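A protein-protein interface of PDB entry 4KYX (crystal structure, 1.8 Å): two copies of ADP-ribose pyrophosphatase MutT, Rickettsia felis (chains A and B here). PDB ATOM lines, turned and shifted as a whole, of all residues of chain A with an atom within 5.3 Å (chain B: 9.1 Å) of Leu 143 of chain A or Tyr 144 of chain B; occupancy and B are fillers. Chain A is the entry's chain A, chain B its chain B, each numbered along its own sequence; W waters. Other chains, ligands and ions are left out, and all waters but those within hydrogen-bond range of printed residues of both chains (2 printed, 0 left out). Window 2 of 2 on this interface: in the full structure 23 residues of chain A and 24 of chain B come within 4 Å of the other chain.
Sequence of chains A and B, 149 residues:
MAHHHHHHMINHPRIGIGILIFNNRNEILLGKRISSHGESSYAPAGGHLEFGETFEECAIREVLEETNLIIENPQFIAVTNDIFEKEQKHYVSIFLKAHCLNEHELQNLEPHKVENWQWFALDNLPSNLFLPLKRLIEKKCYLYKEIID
OH of Tyr 142 of chain A lies within hydrogen-bond range of OE2 of Glu 56 of chain B, 2.6 Å away.
OH of Tyr 144 of chain A lies within hydrogen-bond range of O of Tyr 142 of chain B (3.0 Å).
The backbone NH (N) of Tyr 144 of chain A lies within hydrogen-bond range of the backbone carbonyl oxygen (O) of Ile 77 of chain A, at 2.8 Å.
O of Val 79 of chain A lies within hydrogen-bond range of N of Tyr 142 of chain A, 3.0 Å away.
N of Tyr 144 of chain B sits at hydrogen-bond distance from O of Ile 77 of chain B (2.8 Å).
The backbone carbonyl oxygen (O) of Val 79 of chain B lies within hydrogen-bond range of the backbone NH (N) of Tyr 142 of chain B (3.0 Å).
Val 79 of chain B touches Val 79 of chain A.
Phe 76 of chain B touches Tyr 142 of chain A.
C of Tyr 142 of chain A touches CE1 of Tyr 144 of chain B, 3.8 Å away.
Tyr 144 of chain B touches Leu 143 of chain A.
OH of Tyr 144 of chain A touches CE1 of Phe 76 of chain B (3.5 Å).
Val 79 of chain B touches Tyr 144 of chain A.
Tyr 144 of chain A touches Leu 143 of chain B (CE2 to C, 3.7 Å).
CZ of Tyr 144 of chain A touches CB of Tyr 144 of chain B, 3.6 Å away.
Of chain B, only Tyr 144 (3.2 Å) comes within 4 Å of Leu 143 of chain A.
Of chain A, only Tyr 142, Leu 143 and Tyr 144 come within 4 Å of Tyr 144 of chain B.
Of the printed residues of chain A, Phe 76 of chain B touches Tyr 142 and Tyr 144.
Of the printed residues of chain A, Val 79 of chain B touches Val 79 (3.9 Å) and Tyr 144 (3.7 Å).
Of the printed residues of chain B, Tyr 142 of chain A touches Glu 56 (2.6 Å), Phe 76 (3.7 Å) and Tyr 144 (3.8 Å).
Of the printed residues of chain B, Val 79 of chain A touches Val 79 (3.9 Å).
Printed residues of chain A within 4 Å of Glu 56 of chain B: Tyr 142.
Ile 147 of chain B touches none of the printed residues of chain A.
The nearest residue of chain B that does not touch Leu 143 of chain A is Phe 76 of chain B (6.5 Å).
Of the 20 printed residues of chain B, 6 touch a printed residue of chain A.
Hydrophobic or aromatic side chains of chain B that line the printed part of chain A: Phe 76, Val 79, Tyr 142 and Tyr 144.
Of the 11 printed residues of chain A, 4 touch a printed residue of chain B.
Hydrophobic or aromatic side chains of chain A within 4 Å of the printed part of chain B: Val 79, Tyr 142 and Tyr 144.
Val 79 of chain B touches its own counterpart, Val 79 of chain A.
Tyr 142 of chain A touches Tyr 144 of chain B, and with the chains exchanged Tyr 144 of chain A touches Tyr 142 of chain B.
Leu 143 of chain A touches Tyr 144 of chain B, and with the chains exchanged Tyr 144 of chain A touches Leu 143 of chain B.
Tyr 144 of chain B touches its own counterpart, Tyr 144 of chain A.
Positions printed for both chains: 77, 78, 79, 136, 141, 142, 143, 144, 145 and 146.
Water W1 lies within hydrogen-bond range of OH of Tyr 144 of chain B (2.7 Å), N of Leu 143 of chain A (2.9 Å) and O of Cys 141 of chain A (3.3 Å).
Water W2 bridges OH of Tyr 142 of chain A (2.8 Å) and OE1 of Glu 56 of chain B (3.3 Å).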
ATOM      1  N   ILE A  77     -25.008 -16.452 -20.070  1.00  0.00           N
ATOM      2  CA  ILE A  77     -23.804 -17.238 -20.384  1.00  0.00           C
ATOM      3  C   ILE A  77     -22.617 -16.933 -19.458  1.00  0.00           C
ATOM      4  O   ILE A  77     -21.872 -17.814 -19.087  1.00  0.00           O
ATOM      5  CB  ILE A  77     -23.308 -16.978 -21.833  1.00  0.00           C
ATOM      6  CG1 ILE A  77     -24.316 -17.474 -22.884  1.00  0.00           C
ATOM      7  CG2 ILE A  77     -21.930 -17.600 -22.086  1.00  0.00           C
ATOM      8  CD1 ILE A  77     -24.624 -18.960 -22.866  1.00  0.00           C
ATOM      9  N   ALA A  78     -22.411 -15.658 -19.154  1.00  0.00           N
ATOM     10  CA  ALA A  78     -21.144 -15.285 -18.532  1.00  0.00           C
ATOM     11  C   ALA A  78     -21.118 -13.881 -17.968  1.00  0.00           C
ATOM     12  O   ALA A  78     -21.941 -13.049 -18.303  1.00  0.00           O
ATOM     13  CB  ALA A  78     -20.023 -15.467 -19.520  1.00  0.00           C
ATOM     14  N   VAL A  79     -20.207 -13.664 -17.024  1.00  0.00           N
ATOM     15  CA  VAL A  79     -19.908 -12.331 -16.500  1.00  0.00           C
ATOM     16  C   VAL A  79     -18.435 -12.086 -16.654  1.00  0.00           C
ATOM     17  O   VAL A  79     -17.593 -12.952 -16.347  1.00  0.00           O
ATOM     18  CB  VAL A  79     -20.199 -12.184 -14.977  1.00  0.00           C
ATOM     19  CG1 VAL A  79     -19.941 -10.743 -14.536  1.00  0.00           C
ATOM     20  CG2 VAL A  79     -21.638 -12.591 -14.659  1.00  0.00           C
ATOM     21  N   LEU A 136     -14.345 -13.650 -22.799  1.00  0.00           N
ATOM     22  CA  LEU A 136     -15.298 -14.707 -22.898  1.00  0.00           C
ATOM     23  C   LEU A 136     -14.791 -15.875 -23.764  1.00  0.00           C
ATOM     24  O   LEU A 136     -14.835 -17.051 -23.374  1.00  0.00           O
ATOM     25  CB  LEU A 136     -16.595 -14.146 -23.432  1.00  0.00           C
ATOM     26  CG  LEU A 136     -17.620 -15.220 -23.734  1.00  0.00           C
ATOM     27  CD1 LEU A 136     -17.975 -15.901 -22.436  1.00  0.00           C
ATOM     28  CD2 LEU A 136     -18.861 -14.683 -24.398  1.00  0.00           C
ATOM     29  N   LYS A 139     -12.194 -17.940 -22.244  1.00  0.00           N
ATOM     30  CA  LYS A 139     -12.697 -18.335 -20.923  1.00  0.00           C
ATOM     31  C   LYS A 139     -12.011 -17.671 -19.706  1.00  0.00           C
ATOM     32  O   LYS A 139     -11.907 -18.291 -18.633  1.00  0.00           O
ATOM     33  CB  LYS A 139     -12.602 -19.847 -20.771  1.00  0.00           C
ATOM     34  CG  LYS A 139     -13.205 -20.664 -21.894  1.00  0.00           C
ATOM     35  CD  LYS A 139     -13.264 -22.127 -21.451  1.00  0.00           C
ATOM     36  CE  LYS A 139     -13.300 -23.100 -22.612  1.00  0.00           C
ATOM     37  NZ  LYS A 139     -14.523 -22.886 -23.424  1.00  0.00           N
ATOM     38  N   CYS A 141     -13.277 -15.538 -17.623  1.00  0.00           N
ATOM     39  CA  CYS A 141     -14.540 -14.943 -17.192  1.00  0.00           C
ATOM     40  C   CYS A 141     -15.190 -15.913 -16.219  1.00  0.00           C
ATOM     41  O   CYS A 141     -14.616 -16.952 -15.923  1.00  0.00           O
ATOM     42  CB  CYS A 141     -15.458 -14.688 -18.375  1.00  0.00           C
ATOM     43  SG  CYS A 141     -15.842 -16.203 -19.283  1.00  0.00           S
ATOM     44  N   TYR A 142     -16.369 -15.571 -15.722  1.00  0.00           N
ATOM     45  CA  TYR A 142     -17.159 -16.483 -14.893  1.00  0.00           C
ATOM     46  C   TYR A 142     -18.213 -17.108 -15.829  1.00  0.00           C
ATOM     47  O   TYR A 142     -19.236 -16.485 -16.145  1.00  0.00           O
ATOM     48  CB  TYR A 142     -17.823 -15.709 -13.760  1.00  0.00           C
ATOM     49  CG  TYR A 142     -16.838 -14.912 -12.906  1.00  0.00           C
ATOM     50  CD1 TYR A 142     -16.153 -15.512 -11.830  1.00  0.00           C
ATOM     51  CD2 TYR A 142     -16.554 -13.574 -13.209  1.00  0.00           C
ATOM     52  CE1 TYR A 142     -15.257 -14.792 -11.076  1.00  0.00           C
ATOM     53  CE2 TYR A 142     -15.657 -12.859 -12.445  1.00  0.00           C
ATOM     54  CZ  TYR A 142     -15.030 -13.468 -11.356  1.00  0.00           C
ATOM     55  OH  TYR A 142     -14.142 -12.721 -10.620  1.00  0.00           O
ATOM     56  N   LEU A 143     -17.938 -18.326 -16.291  1.00  0.00           N
ATOM     57  CA  LEU A 143     -18.658 -18.927 -17.429  1.00  0.00           C
ATOM     58  C   LEU A 143     -19.700 -19.880 -16.875  1.00  0.00           C
ATOM     59  O   LEU A 143     -19.377 -20.869 -16.190  1.00  0.00           O
ATOM     60  CB  LEU A 143     -17.685 -19.675 -18.334  1.00  0.00           C
ATOM     61  CG  LEU A 143     -18.243 -20.262 -19.617  1.00  0.00           C
ATOM     62  CD1 LEU A 143     -18.480 -19.135 -20.606  1.00  0.00           C
ATOM     63  CD2 LEU A 143     -17.285 -21.266 -20.265  1.00  0.00           C
ATOM     64  N   TYR A 144     -20.954 -19.532 -17.079  1.00  0.00           N
ATOM     65  CA  TYR A 144     -22.094 -20.342 -16.626  1.00  0.00           C
ATOM     66  C   TYR A 144     -22.337 -21.529 -17.554  1.00  0.00           C
ATOM     67  O   TYR A 144     -22.574 -22.641 -17.090  1.00  0.00           O
ATOM     68  CB  TYR A 144     -23.347 -19.489 -16.634  1.00  0.00           C
ATOM     69  CG  TYR A 144     -23.469 -18.611 -15.449  1.00  0.00           C
ATOM     70  CD1 TYR A 144     -22.458 -17.680 -15.153  1.00  0.00           C
ATOM     71  CD2 TYR A 144     -24.559 -18.730 -14.586  1.00  0.00           C
ATOM     72  CE1 TYR A 144     -22.536 -16.859 -14.069  1.00  0.00           C
ATOM     73  CE2 TYR A 144     -24.658 -17.900 -13.486  1.00  0.00           C
ATOM     74  CZ  TYR A 144     -23.635 -16.978 -13.238  1.00  0.00           C
ATOM     75  OH  TYR A 144     -23.704 -16.168 -12.164  1.00  0.00           O
ATOM     76  N   LYS A 145     -22.318 -21.245 -18.854  1.00  0.00           N
ATOM     77  CA  LYS A 145     -22.628 -22.216 -19.935  1.00  0.00           C
ATOM     78  C   LYS A 145     -21.668 -22.033 -21.103  1.00  0.00           C
ATOM     79  O   LYS A 145     -21.286 -20.906 -21.448  1.00  0.00           O
ATOM     80  CB  LYS A 145     -24.073 -22.010 -20.446  1.00  0.00           C
ATOM     81  N   GLU A 146     -21.300 -23.130 -21.757  1.00  0.00           N
ATOM     82  CA  GLU A 146     -20.436 -23.034 -22.936  1.00  0.00           C
ATOM     83  C   GLU A 146     -21.268 -22.347 -24.019  1.00  0.00           C
ATOM     84  O   GLU A 146     -22.499 -22.445 -24.016  1.00  0.00           O
ATOM     85  CB  GLU A 146     -19.926 -24.408 -23.396  1.00  0.00           C
ATOM     86  CG  GLU A 146     -19.077 -25.178 -22.382  1.00  0.00           C
ATOM     87  CD  GLU A 146     -17.713 -24.560 -22.085  1.00  0.00           C
ATOM     88  OE1 GLU A 146     -17.094 -23.919 -22.979  1.00  0.00           O
ATOM     89  OE2 GLU A 146     -17.232 -24.737 -20.949  1.00  0.00           O
ATOM     90  N   GLU B  56     -13.131 -10.338  -6.231  1.00  0.00           N
ATOM     91  CA  GLU B  56     -12.473 -10.988  -5.131  1.00  0.00           C
ATOM     92  C   GLU B  56     -11.760  -9.976  -4.262  1.00  0.00           C
ATOM     93  O   GLU B  56     -11.816 -10.076  -3.037  1.00  0.00           O
ATOM     94  CB  GLU B  56     -11.480 -12.030  -5.658  1.00  0.00           C
ATOM     95  CG  GLU B  56     -12.122 -13.195  -6.409  1.00  0.00           C
ATOM     96  CD  GLU B  56     -12.500 -12.888  -7.862  1.00  0.00           C
ATOM     97  OE1 GLU B  56     -12.153 -11.842  -8.488  1.00  0.00           O
ATOM     98  OE2 GLU B  56     -13.276 -13.713  -8.395  1.00  0.00           O
ATOM     99  N   PRO B  74     -12.187 -15.948  -2.214  1.00  0.00           N
ATOM    100  CA  PRO B  74     -13.624 -15.934  -2.254  1.00  0.00           C
ATOM    101  C   PRO B  74     -14.091 -16.508  -3.585  1.00  0.00           C
ATOM    102  O   PRO B  74     -13.451 -16.288  -4.631  1.00  0.00           O
ATOM    103  CB  PRO B  74     -13.976 -14.442  -2.061  1.00  0.00           C
ATOM    104  CG  PRO B  74     -12.776 -13.695  -2.535  1.00  0.00           C
ATOM    105  CD  PRO B  74     -11.643 -14.575  -2.113  1.00  0.00           C
ATOM    106  N   GLN B  75     -15.156 -17.294  -3.534  1.00  0.00           N
ATOM    107  CA  GLN B  75     -15.688 -17.969  -4.698  1.00  0.00           C
ATOM    108  C   GLN B  75     -16.936 -17.248  -5.212  1.00  0.00           C
ATOM    109  O   GLN B  75     -17.910 -17.068  -4.540  1.00  0.00           O
ATOM    110  CB  GLN B  75     -15.987 -19.435  -4.349  1.00  0.00           C
ATOM    111  CG  GLN B  75     -14.754 -20.238  -3.889  1.00  0.00           C
ATOM    112  CD  GLN B  75     -13.690 -20.415  -4.963  1.00  0.00           C
ATOM    113  OE1 GLN B  75     -12.482 -20.081  -4.764  1.00  0.00           O
ATOM    114  NE2 GLN B  75     -14.105 -20.915  -6.112  1.00  0.00           N
ATOM    115  N   PHE B  76     -16.931 -16.863  -6.467  1.00  0.00           N
ATOM    116  CA  PHE B  76     -18.121 -16.250  -7.046  1.00  0.00           C
ATOM    117  C   PHE B  76     -19.287 -17.241  -7.064  1.00  0.00           C
ATOM    118  O   PHE B  76     -19.121 -18.392  -7.431  1.00  0.00           O
ATOM    119  CB  PHE B  76     -17.693 -15.781  -8.441  1.00  0.00           C
ATOM    120  CG  PHE B  76     -18.777 -15.253  -9.259  1.00  0.00           C
ATOM    121  CD1 PHE B  76     -19.460 -16.074 -10.134  1.00  0.00           C
ATOM    122  CD2 PHE B  76     -19.050 -13.902  -9.257  1.00  0.00           C
ATOM    123  CE1 PHE B  76     -20.471 -15.571 -10.958  1.00  0.00           C
ATOM    124  CE2 PHE B  76     -20.043 -13.387 -10.081  1.00  0.00           C
ATOM    125  CZ  PHE B  76     -20.776 -14.233 -10.914  1.00  0.00           C
ATOM    126  N   ILE B  77     -20.488 -16.859  -6.663  1.00  0.00           N
ATOM    127  CA  ILE B  77     -21.569 -17.820  -6.656  1.00  0.00           C
ATOM    128  C   ILE B  77     -22.842 -17.450  -7.387  1.00  0.00           C
ATOM    129  O   ILE B  77     -23.529 -18.348  -7.820  1.00  0.00           O
ATOM    130  CB  ILE B  77     -21.980 -18.316  -5.264  1.00  0.00           C
ATOM    131  CG1 ILE B  77     -22.452 -17.191  -4.392  1.00  0.00           C
ATOM    132  CG2 ILE B  77     -20.850 -19.097  -4.589  1.00  0.00           C
ATOM    133  CD1 ILE B  77     -23.077 -17.630  -3.045  1.00  0.00           C
ATOM    134  N   ALA B  78     -23.135 -16.158  -7.560  1.00  0.00           N
ATOM    135  CA  ALA B  78     -24.384 -15.776  -8.173  1.00  0.00           C
ATOM    136  C   ALA B  78     -24.441 -14.289  -8.517  1.00  0.00           C
ATOM    137  O   ALA B  78     -23.738 -13.470  -7.961  1.00  0.00           O
ATOM    138  CB  ALA B  78     -25.532 -16.094  -7.228  1.00  0.00           C
ATOM    139  N   VAL B  79     -25.377 -13.967  -9.382  1.00  0.00           N
ATOM    140  CA  VAL B  79     -25.731 -12.576  -9.746  1.00  0.00           C
ATOM    141  C   VAL B  79     -27.214 -12.415  -9.490  1.00  0.00           C
ATOM    142  O   VAL B  79     -27.986 -13.298  -9.845  1.00  0.00           O
ATOM    143  CB  VAL B  79     -25.463 -12.326 -11.220  1.00  0.00           C
ATOM    144  CG1 VAL B  79     -25.847 -10.912 -11.627  1.00  0.00           C
ATOM    145  CG2 VAL B  79     -23.996 -12.568 -11.529  1.00  0.00           C
ATOM    146  N   THR B  80     -27.606 -11.317  -8.866  1.00  0.00           N
ATOM    147  CA  THR B  80     -29.043 -10.927  -8.753  1.00  0.00           C
ATOM    148  C   THR B  80     -29.265  -9.577  -9.356  1.00  0.00           C
ATOM    149  O   THR B  80     -28.314  -8.780  -9.459  1.00  0.00           O
ATOM    150  CB  THR B  80     -29.539 -10.918  -7.280  1.00  0.00           C
ATOM    151  OG1 THR B  80     -28.817  -9.932  -6.528  1.00  0.00           O
ATOM    152  CG2 THR B  80     -29.291 -12.289  -6.653  1.00  0.00           C
ATOM    153  N   ILE B  94     -23.446  -8.976  -7.020  1.00  0.00           N
ATOM    154  CA  ILE B  94     -22.594 -10.085  -7.219  1.00  0.00           C
ATOM    155  C   ILE B  94     -22.299 -10.748  -5.864  1.00  0.00           C
ATOM    156  O   ILE B  94     -21.778 -10.073  -4.963  1.00  0.00           O
ATOM    157  CB  ILE B  94     -21.253  -9.590  -7.782  1.00  0.00           C
ATOM    158  CG1 ILE B  94     -21.471  -8.742  -9.045  1.00  0.00           C
ATOM    159  CG2 ILE B  94     -20.333 -10.768  -7.962  1.00  0.00           C
ATOM    160  CD1 ILE B  94     -21.967  -9.499 -10.234  1.00  0.00           C
ATOM    161  N   PHE B  95     -22.603 -12.032  -5.734  1.00  0.00           N
ATOM    162  CA  PHE B  95     -22.379 -12.748  -4.487  1.00  0.00           C
ATOM    163  C   PHE B  95     -21.205 -13.661  -4.566  1.00  0.00           C
ATOM    164  O   PHE B  95     -20.988 -14.325  -5.579  1.00  0.00           O
ATOM    165  CB  PHE B  95     -23.613 -13.554  -4.082  1.00  0.00           C
ATOM    166  CG  PHE B  95     -24.685 -12.723  -3.519  1.00  0.00           C
ATOM    167  CD1 PHE B  95     -24.698 -12.361  -2.176  1.00  0.00           C
ATOM    168  CD2 PHE B  95     -25.714 -12.298  -4.330  1.00  0.00           C
ATOM    169  CE1 PHE B  95     -25.746 -11.633  -1.648  1.00  0.00           C
ATOM    170  CE2 PHE B  95     -26.734 -11.535  -3.816  1.00  0.00           C
ATOM    171  CZ  PHE B  95     -26.747 -11.181  -2.511  1.00  0.00           C
ATOM    172  N   LEU B  96     -20.377 -13.639  -3.506  1.00  0.00           N
ATOM    173  CA  LEU B  96     -19.269 -14.563  -3.364  1.00  0.00           C
ATOM    174  C   LEU B  96     -19.398 -15.217  -1.977  1.00  0.00           C
ATOM    175  O   LEU B  96     -20.083 -14.693  -1.134  1.00  0.00           O
ATOM    176  CB  LEU B  96     -17.905 -13.847  -3.429  1.00  0.00           C
ATOM    177  CG  LEU B  96     -17.614 -13.115  -4.746  1.00  0.00           C
ATOM    178  CD1 LEU B  96     -18.104 -11.668  -4.630  1.00  0.00           C
ATOM    179  CD2 LEU B  96     -16.151 -13.128  -5.093  1.00  0.00           C
ATOM    180  N   LYS B  97     -18.740 -16.339  -1.819  1.00  0.00           N
ATOM    181  CA  LYS B  97     -18.595 -17.013  -0.564  1.00  0.00           C
ATOM    182  C   LYS B  97     -17.174 -17.306  -0.175  1.00  0.00           C
ATOM    183  O   LYS B  97     -16.279 -17.427  -1.007  1.00  0.00           O
ATOM    184  CB  LYS B  97     -19.372 -18.303  -0.551  1.00  0.00           C
ATOM    185  CG  LYS B  97     -18.808 -19.351  -1.489  1.00  0.00           C
ATOM    186  CD  LYS B  97     -19.635 -20.628  -1.464  1.00  0.00           C
ATOM    187  CE  LYS B  97     -18.921 -21.710  -2.259  1.00  0.00           C
ATOM    188  NZ  LYS B  97     -19.746 -22.945  -2.251  1.00  0.00           N
ATOM    189  N   LEU B 136     -31.204 -14.601  -3.638  1.00  0.00           N
ATOM    190  CA  LEU B 136     -30.195 -15.642  -3.688  1.00  0.00           C
ATOM    191  C   LEU B 136     -30.675 -16.955  -3.053  1.00  0.00           C
ATOM    192  O   LEU B 136     -30.641 -18.013  -3.681  1.00  0.00           O
ATOM    193  CB  LEU B 136     -28.893 -15.144  -3.052  1.00  0.00           C
ATOM    194  CG  LEU B 136     -27.838 -16.211  -2.835  1.00  0.00           C
ATOM    195  CD1 LEU B 136     -27.365 -16.683  -4.197  1.00  0.00           C
ATOM    196  CD2 LEU B 136     -26.704 -15.644  -2.010  1.00  0.00           C
ATOM    197  N   CYS B 141     -32.261 -15.970  -9.112  1.00  0.00           N
ATOM    198  CA  CYS B 141     -30.923 -15.385  -9.421  1.00  0.00           C
ATOM    199  C   CYS B 141     -30.293 -16.223 -10.510  1.00  0.00           C
ATOM    200  O   CYS B 141     -30.903 -17.176 -10.976  1.00  0.00           O
ATOM    201  CB  CYS B 141     -30.039 -15.412  -8.154  1.00  0.00           C
ATOM    202  SG  CYS B 141     -29.688 -17.091  -7.613  1.00  0.00           S
ATOM    203  N   TYR B 142     -29.078 -15.858 -10.928  1.00  0.00           N
ATOM    204  CA  TYR B 142     -28.325 -16.619 -11.895  1.00  0.00           C
ATOM    205  C   TYR B 142     -27.222 -17.265 -11.072  1.00  0.00           C
ATOM    206  O   TYR B 142     -26.255 -16.622 -10.674  1.00  0.00           O
ATOM    207  CB  TYR B 142     -27.779 -15.698 -12.981  1.00  0.00           C
ATOM    208  CG  TYR B 142     -28.851 -14.906 -13.675  1.00  0.00           C
ATOM    209  CD1 TYR B 142     -29.504 -15.393 -14.829  1.00  0.00           C
ATOM    210  CD2 TYR B 142     -29.218 -13.666 -13.195  1.00  0.00           C
ATOM    211  CE1 TYR B 142     -30.473 -14.641 -15.437  1.00  0.00           C
ATOM    212  CE2 TYR B 142     -30.198 -12.921 -13.783  1.00  0.00           C
ATOM    213  CZ  TYR B 142     -30.812 -13.399 -14.931  1.00  0.00           C
ATOM    214  OH  TYR B 142     -31.777 -12.603 -15.546  1.00  0.00           O
ATOM    215  N   LEU B 143     -27.444 -18.534 -10.761  1.00  0.00           N
ATOM    216  CA  LEU B 143     -26.599 -19.289  -9.826  1.00  0.00           C
ATOM    217  C   LEU B 143     -25.457 -19.992 -10.537  1.00  0.00           C
ATOM    218  O   LEU B 143     -25.668 -20.824 -11.434  1.00  0.00           O
ATOM    219  CB  LEU B 143     -27.470 -20.288  -9.045  1.00  0.00           C
ATOM    220  CG  LEU B 143     -26.796 -20.938  -7.831  1.00  0.00           C
ATOM    221  CD1 LEU B 143     -26.578 -19.919  -6.714  1.00  0.00           C
ATOM    222  CD2 LEU B 143     -27.627 -22.109  -7.337  1.00  0.00           C
ATOM    223  N   TYR B 144     -24.243 -19.603 -10.185  1.00  0.00           N
ATOM    224  CA  TYR B 144     -23.009 -20.122 -10.783  1.00  0.00           C
ATOM    225  C   TYR B 144     -22.502 -21.333 -10.019  1.00  0.00           C
ATOM    226  O   TYR B 144     -22.000 -22.254 -10.642  1.00  0.00           O
ATOM    227  CB  TYR B 144     -21.942 -19.008 -10.818  1.00  0.00           C
ATOM    228  CG  TYR B 144     -20.585 -19.341 -11.367  1.00  0.00           C
ATOM    229  CD1 TYR B 144     -20.367 -19.436 -12.724  1.00  0.00           C
ATOM    230  CD2 TYR B 144     -19.482 -19.482 -10.516  1.00  0.00           C
ATOM    231  CE1 TYR B 144     -19.096 -19.717 -13.237  1.00  0.00           C
ATOM    232  CE2 TYR B 144     -18.213 -19.761 -11.016  1.00  0.00           C
ATOM    233  CZ  TYR B 144     -18.028 -19.870 -12.390  1.00  0.00           C
ATOM    234  OH  TYR B 144     -16.788 -20.117 -12.902  1.00  0.00           O
ATOM    235  N   LYS B 145     -22.629 -21.301  -8.689  1.00  0.00           N
ATOM    236  CA  LYS B 145     -22.344 -22.399  -7.766  1.00  0.00           C
ATOM    237  C   LYS B 145     -23.307 -22.398  -6.563  1.00  0.00           C
ATOM    238  O   LYS B 145     -23.797 -21.344  -6.148  1.00  0.00           O
ATOM    239  CB  LYS B 145     -20.899 -22.293  -7.209  1.00  0.00           C
ATOM    240  N   GLU B 146     -23.536 -23.575  -5.978  1.00  0.00           N
ATOM    241  CA  GLU B 146     -24.398 -23.705  -4.795  1.00  0.00           C
ATOM    242  C   GLU B 146     -23.736 -23.019  -3.595  1.00  0.00           C
ATOM    243  O   GLU B 146     -22.511 -22.904  -3.541  1.00  0.00           O
ATOM    244  CB  GLU B 146     -24.673 -25.182  -4.441  1.00  0.00           C
ATOM    245  CG  GLU B 146     -25.518 -25.960  -5.463  1.00  0.00           C
ATOM    246  CD  GLU B 146     -26.928 -25.425  -5.623  1.00  0.00           C
ATOM    247  OE1 GLU B 146     -27.476 -24.838  -4.668  1.00  0.00           O
ATOM    248  OE2 GLU B 146     -27.501 -25.599  -6.715  1.00  0.00           O
ATOM    249  N   ILE B 147     -24.553 -22.554  -2.661  1.00  0.00           N
ATOM    250  CA  ILE B 147     -24.065 -21.932  -1.429  1.00  0.00           C
ATOM    251  C   ILE B 147     -23.258 -22.931  -0.592  1.00  0.00           C
ATOM    252  O   ILE B 147     -22.247 -22.582   0.022  1.00  0.00           O
ATOM    253  CB  ILE B 147     -25.237 -21.344  -0.612  1.00  0.00           C
ATOM    254  CG1 ILE B 147     -25.824 -20.127  -1.335  1.00  0.00           C
ATOM    255  CG2 ILE B 147     -24.799 -20.921   0.777  1.00  0.00           C
ATOM    256  CD1 ILE B 147     -27.014 -19.540  -0.605  1.00  0.00           C
HETATM  257  O   HOH W   1     -15.772 -19.989 -15.371  1.00  0.00           O
HETATM  258  O   HOH W   2     -13.562  -9.974 -10.877  1.00  0.00           O
